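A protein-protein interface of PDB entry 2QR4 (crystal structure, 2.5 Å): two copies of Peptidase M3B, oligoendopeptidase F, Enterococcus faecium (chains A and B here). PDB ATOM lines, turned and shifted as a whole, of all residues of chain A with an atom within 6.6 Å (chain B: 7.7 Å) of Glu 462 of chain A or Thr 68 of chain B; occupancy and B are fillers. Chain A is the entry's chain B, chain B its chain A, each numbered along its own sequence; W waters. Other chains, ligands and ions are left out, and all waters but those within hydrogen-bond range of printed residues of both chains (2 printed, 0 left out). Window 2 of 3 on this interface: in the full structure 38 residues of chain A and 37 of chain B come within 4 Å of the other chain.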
ATOM      1  N   ARG A 208       6.619  13.972  -4.881  1.00  0.00           N
ATOM      2  CA  ARG A 208       6.540  12.713  -4.146  1.00  0.00           C
ATOM      3  C   ARG A 208       6.235  11.506  -5.059  1.00  0.00           C
ATOM      4  O   ARG A 208       6.739  10.417  -4.832  1.00  0.00           O
ATOM      5  CB  ARG A 208       5.519  12.834  -3.005  1.00  0.00           C
ATOM      6  CG  ARG A 208       4.087  12.691  -3.427  1.00  0.00           C
ATOM      7  CD  ARG A 208       3.122  13.082  -2.330  1.00  0.00           C
ATOM      8  NE  ARG A 208       2.667  14.444  -2.535  1.00  0.00           N
ATOM      9  CZ  ARG A 208       1.445  14.775  -2.927  1.00  0.00           C
ATOM     10  NH1 ARG A 208       0.532  13.846  -3.112  1.00  0.00           N
ATOM     11  NH2 ARG A 208       1.133  16.048  -3.100  1.00  0.00           N
ATOM     12  N   ASN A 209       5.430  11.700  -6.098  1.00  0.00           N
ATOM     13  CA  ASN A 209       5.103  10.610  -7.022  1.00  0.00           C
ATOM     14  C   ASN A 209       6.296  10.160  -7.873  1.00  0.00           C
ATOM     15  O   ASN A 209       6.547   8.960  -8.039  1.00  0.00           O
ATOM     16  CB  ASN A 209       3.942  11.017  -7.925  1.00  0.00           C
ATOM     17  CG  ASN A 209       2.627  11.149  -7.168  1.00  0.00           C
ATOM     18  OD1 ASN A 209       2.262  10.279  -6.380  1.00  0.00           O
ATOM     19  ND2 ASN A 209       1.911  12.237  -7.411  1.00  0.00           N
ATOM     20  N   ALA A 212       8.744   8.376  -5.618  1.00  0.00           N
ATOM     21  CA  ALA A 212       8.221   7.065  -5.220  1.00  0.00           C
ATOM     22  C   ALA A 212       8.511   6.074  -6.326  1.00  0.00           C
ATOM     23  O   ALA A 212       8.854   4.924  -6.072  1.00  0.00           O
ATOM     24  CB  ALA A 212       6.732   7.125  -4.976  1.00  0.00           C
ATOM     25  N   LEU A 459       4.331   0.464  -3.428  1.00  0.00           N
ATOM     26  CA  LEU A 459       4.986   1.539  -2.705  1.00  0.00           C
ATOM     27  C   LEU A 459       4.613   2.888  -3.321  1.00  0.00           C
ATOM     28  O   LEU A 459       5.475   3.616  -3.829  1.00  0.00           O
ATOM     29  CB  LEU A 459       6.506   1.336  -2.735  1.00  0.00           C
ATOM     30  CG  LEU A 459       7.218   0.670  -1.535  1.00  0.00           C
ATOM     31  CD1 LEU A 459       6.360  -0.271  -0.755  1.00  0.00           C
ATOM     32  CD2 LEU A 459       8.502  -0.034  -1.966  1.00  0.00           C
ATOM     33  N   THR A 460       3.323   3.208  -3.292  1.00  0.00           N
ATOM     34  CA  THR A 460       2.841   4.503  -3.758  1.00  0.00           C
ATOM     35  C   THR A 460       3.357   5.583  -2.819  1.00  0.00           C
ATOM     36  O   THR A 460       3.737   5.310  -1.677  1.00  0.00           O
ATOM     37  CB  THR A 460       1.314   4.548  -3.768  1.00  0.00           C
ATOM     38  OG1 THR A 460       0.826   4.400  -2.428  1.00  0.00           O
ATOM     39  CG2 THR A 460       0.761   3.420  -4.614  1.00  0.00           C
ATOM     40  N   SER A 461       3.374   6.818  -3.285  1.00  0.00           N
ATOM     41  CA  SER A 461       3.935   7.865  -2.471  1.00  0.00           C
ATOM     42  C   SER A 461       3.074   8.089  -1.234  1.00  0.00           C
ATOM     43  O   SER A 461       3.596   8.433  -0.175  1.00  0.00           O
ATOM     44  CB  SER A 461       4.077   9.157  -3.276  1.00  0.00           C
ATOM     45  OG  SER A 461       2.808   9.704  -3.571  1.00  0.00           O
ATOM     46  N   GLU A 462       1.761   7.903  -1.363  1.00  0.00           N
ATOM     47  CA  GLU A 462       0.886   8.074  -0.206  1.00  0.00           C
ATOM     48  C   GLU A 462       1.237   7.085   0.902  1.00  0.00           C
ATOM     49  O   GLU A 462       1.361   7.468   2.062  1.00  0.00           O
ATOM     50  CB  GLU A 462      -0.591   7.953  -0.575  1.00  0.00           C
ATOM     51  CG  GLU A 462      -1.527   8.104   0.634  1.00  0.00           C
ATOM     52  CD  GLU A 462      -2.959   8.526   0.256  1.00  0.00           C
ATOM     53  OE1 GLU A 462      -3.561   9.308   1.020  1.00  0.00           O
ATOM     54  OE2 GLU A 462      -3.489   8.098  -0.795  1.00  0.00           O
ATOM     55  N   TYR A 463       1.414   5.818   0.535  1.00  0.00           N
ATOM     56  CA  TYR A 463       1.762   4.778   1.496  1.00  0.00           C
ATOM     57  C   TYR A 463       3.155   4.993   2.103  1.00  0.00           C
ATOM     58  O   TYR A 463       3.360   4.835   3.309  1.00  0.00           O
ATOM     59  CB  TYR A 463       1.668   3.403   0.831  1.00  0.00           C
ATOM     60  CG  TYR A 463       1.927   2.246   1.769  1.00  0.00           C
ATOM     61  CD1 TYR A 463       1.142   2.055   2.906  1.00  0.00           C
ATOM     62  CD2 TYR A 463       2.952   1.333   1.512  1.00  0.00           C
ATOM     63  CE1 TYR A 463       1.379   0.990   3.783  1.00  0.00           C
ATOM     64  CE2 TYR A 463       3.191   0.263   2.367  1.00  0.00           C
ATOM     65  CZ  TYR A 463       2.400   0.100   3.500  1.00  0.00           C
ATOM     66  OH  TYR A 463       2.641  -0.959   4.338  1.00  0.00           O
ATOM     67  N   LEU A 464       4.114   5.343   1.261  1.00  0.00           N
ATOM     68  CA  LEU A 464       5.468   5.608   1.715  1.00  0.00           C
ATOM     69  C   LEU A 464       5.442   6.747   2.736  1.00  0.00           C
ATOM     70  O   LEU A 464       6.043   6.666   3.812  1.00  0.00           O
ATOM     71  CB  LEU A 464       6.314   6.024   0.526  1.00  0.00           C
ATOM     72  CG  LEU A 464       7.385   5.141  -0.111  1.00  0.00           C
ATOM     73  CD1 LEU A 464       7.457   3.755   0.447  1.00  0.00           C
ATOM     74  CD2 LEU A 464       7.228   5.131  -1.612  1.00  0.00           C
ATOM     75  N   SER A 465       4.720   7.803   2.400  1.00  0.00           N
ATOM     76  CA  SER A 465       4.678   8.997   3.232  1.00  0.00           C
ATOM     77  C   SER A 465       3.911   8.793   4.540  1.00  0.00           C
ATOM     78  O   SER A 465       4.316   9.308   5.597  1.00  0.00           O
ATOM     79  CB  SER A 465       4.092  10.156   2.433  1.00  0.00           C
ATOM     80  OG  SER A 465       4.825  10.326   1.223  1.00  0.00           O
ATOM     81  N   ASP A 466       2.804   8.057   4.476  1.00  0.00           N
ATOM     82  CA  ASP A 466       2.067   7.744   5.694  1.00  0.00           C
ATOM     83  C   ASP A 466       2.936   6.874   6.590  1.00  0.00           C
ATOM     84  O   ASP A 466       3.106   7.170   7.774  1.00  0.00           O
ATOM     85  CB  ASP A 466       0.731   7.051   5.402  1.00  0.00           C
ATOM     86  CG  ASP A 466      -0.339   8.016   4.924  1.00  0.00           C
ATOM     87  OD1 ASP A 466      -0.156   9.250   5.050  1.00  0.00           O
ATOM     88  OD2 ASP A 466      -1.377   7.535   4.420  1.00  0.00           O
ATOM     89  N   SER A 467       3.504   5.817   6.019  1.00  0.00           N
ATOM     90  CA  SER A 467       4.372   4.938   6.787  1.00  0.00           C
ATOM     91  C   SER A 467       5.572   5.711   7.354  1.00  0.00           C
ATOM     92  O   SER A 467       5.962   5.471   8.490  1.00  0.00           O
ATOM     93  CB  SER A 467       4.868   3.764   5.948  1.00  0.00           C
ATOM     94  OG  SER A 467       3.819   3.104   5.265  1.00  0.00           O
ATOM     95  N   TRP A 490      11.425  10.785   3.295  1.00  0.00           N
ATOM     96  CA  TRP A 490      11.949   9.577   2.613  1.00  0.00           C
ATOM     97  C   TRP A 490      12.471   9.864   1.205  1.00  0.00           C
ATOM     98  O   TRP A 490      13.365   9.177   0.718  1.00  0.00           O
ATOM     99  CB  TRP A 490      10.905   8.455   2.561  1.00  0.00           C
ATOM    100  CG  TRP A 490       9.660   8.854   1.828  1.00  0.00           C
ATOM    101  CD1 TRP A 490       8.520   9.371   2.371  1.00  0.00           C
ATOM    102  CD2 TRP A 490       9.438   8.789   0.414  1.00  0.00           C
ATOM    103  NE1 TRP A 490       7.604   9.640   1.383  1.00  0.00           N
ATOM    104  CE2 TRP A 490       8.144   9.291   0.172  1.00  0.00           C
ATOM    105  CE3 TRP A 490      10.208   8.348  -0.674  1.00  0.00           C
ATOM    106  CZ2 TRP A 490       7.599   9.368  -1.113  1.00  0.00           C
ATOM    107  CZ3 TRP A 490       9.662   8.428  -1.958  1.00  0.00           C
ATOM    108  CH2 TRP A 490       8.375   8.928  -2.165  1.00  0.00           C
ATOM    109  N   ASN B  61      -4.456   4.109 -15.022  1.00  0.00           N
ATOM    110  CA  ASN B  61      -3.331   4.861 -14.492  1.00  0.00           C
ATOM    111  C   ASN B  61      -3.076   6.112 -15.327  1.00  0.00           C
ATOM    112  O   ASN B  61      -2.994   7.220 -14.794  1.00  0.00           O
ATOM    113  CB  ASN B  61      -2.079   3.993 -14.471  1.00  0.00           C
ATOM    114  CG  ASN B  61      -0.924   4.647 -13.732  1.00  0.00           C
ATOM    115  OD1 ASN B  61       0.207   4.687 -14.221  1.00  0.00           O
ATOM    116  ND2 ASN B  61      -1.201   5.144 -12.541  1.00  0.00           N
ATOM    117  N   ASP B  64      -5.573   9.100 -14.737  1.00  0.00           N
ATOM    118  CA  ASP B  64      -5.320   9.940 -13.559  1.00  0.00           C
ATOM    119  C   ASP B  64      -4.110   9.412 -12.776  1.00  0.00           C
ATOM    120  O   ASP B  64      -4.265   8.698 -11.785  1.00  0.00           O
ATOM    121  CB  ASP B  64      -6.565  10.004 -12.674  1.00  0.00           C
ATOM    122  CG  ASP B  64      -6.422  10.975 -11.514  1.00  0.00           C
ATOM    123  OD1 ASP B  64      -5.342  11.587 -11.348  1.00  0.00           O
ATOM    124  OD2 ASP B  64      -7.407  11.124 -10.758  1.00  0.00           O
ATOM    125  N   THR B  65      -2.911   9.772 -13.229  1.00  0.00           N
ATOM    126  CA  THR B  65      -1.677   9.185 -12.697  1.00  0.00           C
ATOM    127  C   THR B  65      -1.355   9.634 -11.279  1.00  0.00           C
ATOM    128  O   THR B  65      -0.493   9.055 -10.628  1.00  0.00           O
ATOM    129  CB  THR B  65      -0.458   9.456 -13.602  1.00  0.00           C
ATOM    130  OG1 THR B  65      -0.864   9.480 -14.971  1.00  0.00           O
ATOM    131  CG2 THR B  65       0.579   8.349 -13.423  1.00  0.00           C
ATOM    132  N   GLY B  66      -2.047  10.664 -10.805  1.00  0.00           N
ATOM    133  CA  GLY B  66      -1.864  11.133  -9.443  1.00  0.00           C
ATOM    134  C   GLY B  66      -2.780  10.438  -8.448  1.00  0.00           C
ATOM    135  O   GLY B  66      -2.719  10.708  -7.248  1.00  0.00           O
ATOM    136  N   ASN B  67      -3.625   9.535  -8.938  1.00  0.00           N
ATOM    137  CA  ASN B  67      -4.609   8.854  -8.097  1.00  0.00           C
ATOM    138  C   ASN B  67      -4.050   7.582  -7.435  1.00  0.00           C
ATOM    139  O   ASN B  67      -3.751   6.596  -8.116  1.00  0.00           O
ATOM    140  CB  ASN B  67      -5.864   8.549  -8.920  1.00  0.00           C
ATOM    141  CG  ASN B  67      -6.933   7.815  -8.122  1.00  0.00           C
ATOM    142  OD1 ASN B  67      -6.692   6.743  -7.576  1.00  0.00           O
ATOM    143  ND2 ASN B  67      -8.124   8.385  -8.072  1.00  0.00           N
ATOM    144  N   THR B  68      -3.927   7.614  -6.105  1.00  0.00           N
ATOM    145  CA  THR B  68      -3.351   6.515  -5.325  1.00  0.00           C
ATOM    146  C   THR B  68      -3.949   5.163  -5.681  1.00  0.00           C
ATOM    147  O   THR B  68      -3.221   4.208  -5.942  1.00  0.00           O
ATOM    148  CB  THR B  68      -3.494   6.745  -3.800  1.00  0.00           C
ATOM    149  OG1 THR B  68      -2.713   7.878  -3.417  1.00  0.00           O
ATOM    150  CG2 THR B  68      -2.995   5.533  -3.023  1.00  0.00           C
ATOM    151  N   ASP B  69      -5.273   5.078  -5.704  1.00  0.00           N
ATOM    152  CA  ASP B  69      -5.924   3.816  -6.015  1.00  0.00           C
ATOM    153  C   ASP B  69      -5.561   3.299  -7.393  1.00  0.00           C
ATOM    154  O   ASP B  69      -5.418   2.098  -7.572  1.00  0.00           O
ATOM    155  CB  ASP B  69      -7.434   3.935  -5.864  1.00  0.00           C
ATOM    156  CG  ASP B  69      -7.830   4.259  -4.451  1.00  0.00           C
ATOM    157  OD1 ASP B  69      -8.995   4.650  -4.230  1.00  0.00           O
ATOM    158  OD2 ASP B  69      -6.962   4.126  -3.559  1.00  0.00           O
ATOM    159  N   TYR B  70      -5.382   4.195  -8.359  1.00  0.00           N
ATOM    160  CA  TYR B  70      -4.995   3.751  -9.701  1.00  0.00           C
ATOM    161  C   TYR B  70      -3.535   3.339  -9.722  1.00  0.00           C
ATOM    162  O   TYR B  70      -3.191   2.320 -10.322  1.00  0.00           O
ATOM    163  CB  TYR B  70      -5.249   4.814 -10.776  1.00  0.00           C
ATOM    164  CG  TYR B  70      -6.702   5.220 -10.971  1.00  0.00           C
ATOM    165  CD1 TYR B  70      -7.749   4.410 -10.543  1.00  0.00           C
ATOM    166  CD2 TYR B  70      -7.020   6.411 -11.616  1.00  0.00           C
ATOM    167  CE1 TYR B  70      -9.076   4.795 -10.730  1.00  0.00           C
ATOM    168  CE2 TYR B  70      -8.328   6.799 -11.811  1.00  0.00           C
ATOM    169  CZ  TYR B  70      -9.352   5.994 -11.371  1.00  0.00           C
ATOM    170  OH  TYR B  70     -10.653   6.408 -11.571  1.00  0.00           O
ATOM    171  N   GLN B  71      -2.677   4.121  -9.064  1.00  0.00           N
ATOM    172  CA  GLN B  71      -1.261   3.765  -8.958  1.00  0.00           C
ATOM    173  C   GLN B  71      -1.122   2.337  -8.406  1.00  0.00           C
ATOM    174  O   GLN B  71      -0.377   1.515  -8.948  1.00  0.00           O
ATOM    175  CB  GLN B  71      -0.533   4.731  -8.032  1.00  0.00           C
ATOM    176  CG  GLN B  71      -0.420   6.151  -8.541  1.00  0.00           C
ATOM    177  CD  GLN B  71       0.143   7.082  -7.485  1.00  0.00           C
ATOM    178  OE1 GLN B  71       0.287   6.697  -6.323  1.00  0.00           O
ATOM    179  NE2 GLN B  71       0.454   8.319  -7.877  1.00  0.00           N
ATOM    180  N   ALA B  72      -1.867   2.059  -7.335  1.00  0.00           N
ATOM    181  CA  ALA B  72      -1.839   0.763  -6.654  1.00  0.00           C
ATOM    182  C   ALA B  72      -2.314  -0.371  -7.544  1.00  0.00           C
ATOM    183  O   ALA B  72      -1.708  -1.444  -7.573  1.00  0.00           O
ATOM    184  CB  ALA B  72      -2.686   0.813  -5.396  1.00  0.00           C
ATOM    185  N   LEU B  73      -3.404  -0.125  -8.267  1.00  0.00           N
ATOM    186  CA  LEU B  73      -3.992  -1.123  -9.152  1.00  0.00           C
ATOM    187  C   LEU B  73      -2.995  -1.475 -10.250  1.00  0.00           C
ATOM    188  O   LEU B  73      -2.749  -2.651 -10.533  1.00  0.00           O
ATOM    189  CB  LEU B  73      -5.280  -0.578  -9.753  1.00  0.00           C
ATOM    190  CG  LEU B  73      -6.491  -1.490  -9.899  1.00  0.00           C
ATOM    191  CD1 LEU B  73      -6.372  -2.356 -11.140  1.00  0.00           C
ATOM    192  CD2 LEU B  73      -6.664  -2.338  -8.660  1.00  0.00           C
ATOM    193  N   TYR B  74      -2.389  -0.445 -10.835  1.00  0.00           N
ATOM    194  CA  TYR B  74      -1.435  -0.622 -11.924  1.00  0.00           C
ATOM    195  C   TYR B  74      -0.178  -1.376 -11.464  1.00  0.00           C
ATOM    196  O   TYR B  74       0.326  -2.253 -12.158  1.00  0.00           O
ATOM    197  CB  TYR B  74      -1.086   0.737 -12.544  1.00  0.00           C
ATOM    198  CG  TYR B  74      -0.044   0.677 -13.636  1.00  0.00           C
ATOM    199  CD1 TYR B  74      -0.162  -0.223 -14.695  1.00  0.00           C
ATOM    200  CD2 TYR B  74       1.052   1.535 -13.623  1.00  0.00           C
ATOM    201  CE1 TYR B  74       0.802  -0.289 -15.692  1.00  0.00           C
ATOM    202  CE2 TYR B  74       2.018   1.480 -14.620  1.00  0.00           C
ATOM    203  CZ  TYR B  74       1.890   0.569 -15.649  1.00  0.00           C
ATOM    204  OH  TYR B  74       2.839   0.527 -16.638  1.00  0.00           O
ATOM    205  N   ALA B  75       0.314  -1.042 -10.282  1.00  0.00           N
ATOM    206  CA  ALA B  75       1.430  -1.768  -9.694  1.00  0.00           C
ATOM    207  C   ALA B  75       1.077  -3.242  -9.458  1.00  0.00           C
ATOM    208  O   ALA B  75       1.826  -4.125  -9.845  1.00  0.00           O
ATOM    209  CB  ALA B  75       1.850  -1.100  -8.388  1.00  0.00           C
ATOM    210  N   ARG B  76      -0.071  -3.520  -8.844  1.00  0.00           N
ATOM    211  CA  ARG B  76      -0.448  -4.919  -8.626  1.00  0.00           C
ATOM    212  C   ARG B  76      -0.565  -5.657  -9.956  1.00  0.00           C
ATOM    213  O   ARG B  76      -0.153  -6.812 -10.066  1.00  0.00           O
ATOM    214  CB  ARG B  76      -1.740  -5.048  -7.795  1.00  0.00           C
ATOM    215  CG  ARG B  76      -1.581  -4.564  -6.363  1.00  0.00           C
ATOM    216  CD  ARG B  76      -2.778  -4.878  -5.478  1.00  0.00           C
ATOM    217  NE  ARG B  76      -2.365  -5.052  -4.078  1.00  0.00           N
ATOM    218  CZ  ARG B  76      -2.506  -4.142  -3.107  1.00  0.00           C
ATOM    219  NH1 ARG B  76      -2.085  -4.426  -1.876  1.00  0.00           N
ATOM    220  NH2 ARG B  76      -3.063  -2.952  -3.350  1.00  0.00           N
HETATM  221  O   HOH W   1       0.077   7.910  -3.930  1.00  0.00           O
HETATM  222  O   HOH W   2       3.099   7.107  -6.225  1.00  0.00           O
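The side-chain hydroxyl (OG1) of Thr 68 of chain B lies within hydrogen-bond range of the side-chain carboxylate (OE2) of Glu 462 of chain A, at 2.7 Å. NE2 of Gln 71 of chain B sits at hydrogen-bond distance from OD1 of Asn 209 of chain A (3.1 Å).
Of the 14 printed residues of chain B, 2 touch a printed residue of chain A. Along chain B the printed residues that touch a printed residue of chain A span positions 68 to 71. Among the printed residues, no Asp or Glu carboxylate lies within 4 Å of a Lys or Arg side-chain nitrogen of the other chain.
Among the printed residues, pairs that only touch across the chains: Thr 460 of chain A with Gln 71 of chain B (3.5 Å).
Water W1 lies within hydrogen-bond range of the side-chain amide oxygen (OE1) of Gln 71 of chain B, the side-chain hydroxyl (OG1) of Thr 68 of chain B, the backbone NH (N) of Glu 462 of chain A and the side-chain hydroxyl (OG) of Ser 461 of chain A. Water W2 lies within hydrogen-bond range of the side-chain amide oxygen (OE1) of Gln 71 of chain B (2.8 Å), the backbone NH (N) of Ser 461 of chain A (3.0 Å) and the side-chain amide oxygen (OD1) of Asn 209 of chain A (3.3 Å).
No position is printed for both chains.
Of the printed residues of chain B, Asn 209 of chain A touches Gln 71 (3.1 Å). Ala 212 of chain A touches none of the printed residues of chain B. Of the printed residues of chain B, Thr 460 of chain A touches Gln 71 (3.5 Å). Of the printed residues of chain A, Gln 71 of chain B touches Asn 209 (3.1 Å) and Thr 460 (3.5 Å). Leu 73 of chain B touches none of the printed residues of chain A.
The side-chain amide nitrogen of Gln 71 of chain B sits at hydrogen-bond distance from the backbone carbonyl oxygen of Thr 65 of chain B, 3.0 Å away. The side-chain amide oxygen (OD1) of Asn 209 of chain A is in hydrogen-bond range of the side-chain hydroxyl (OG) of Ser 461 of chain A (2.9 Å). The backbone NH (N) of Tyr 463 of chain A is in hydrogen-bond range of the side-chain hydroxyl (OG1) of Thr 460 of chain A.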
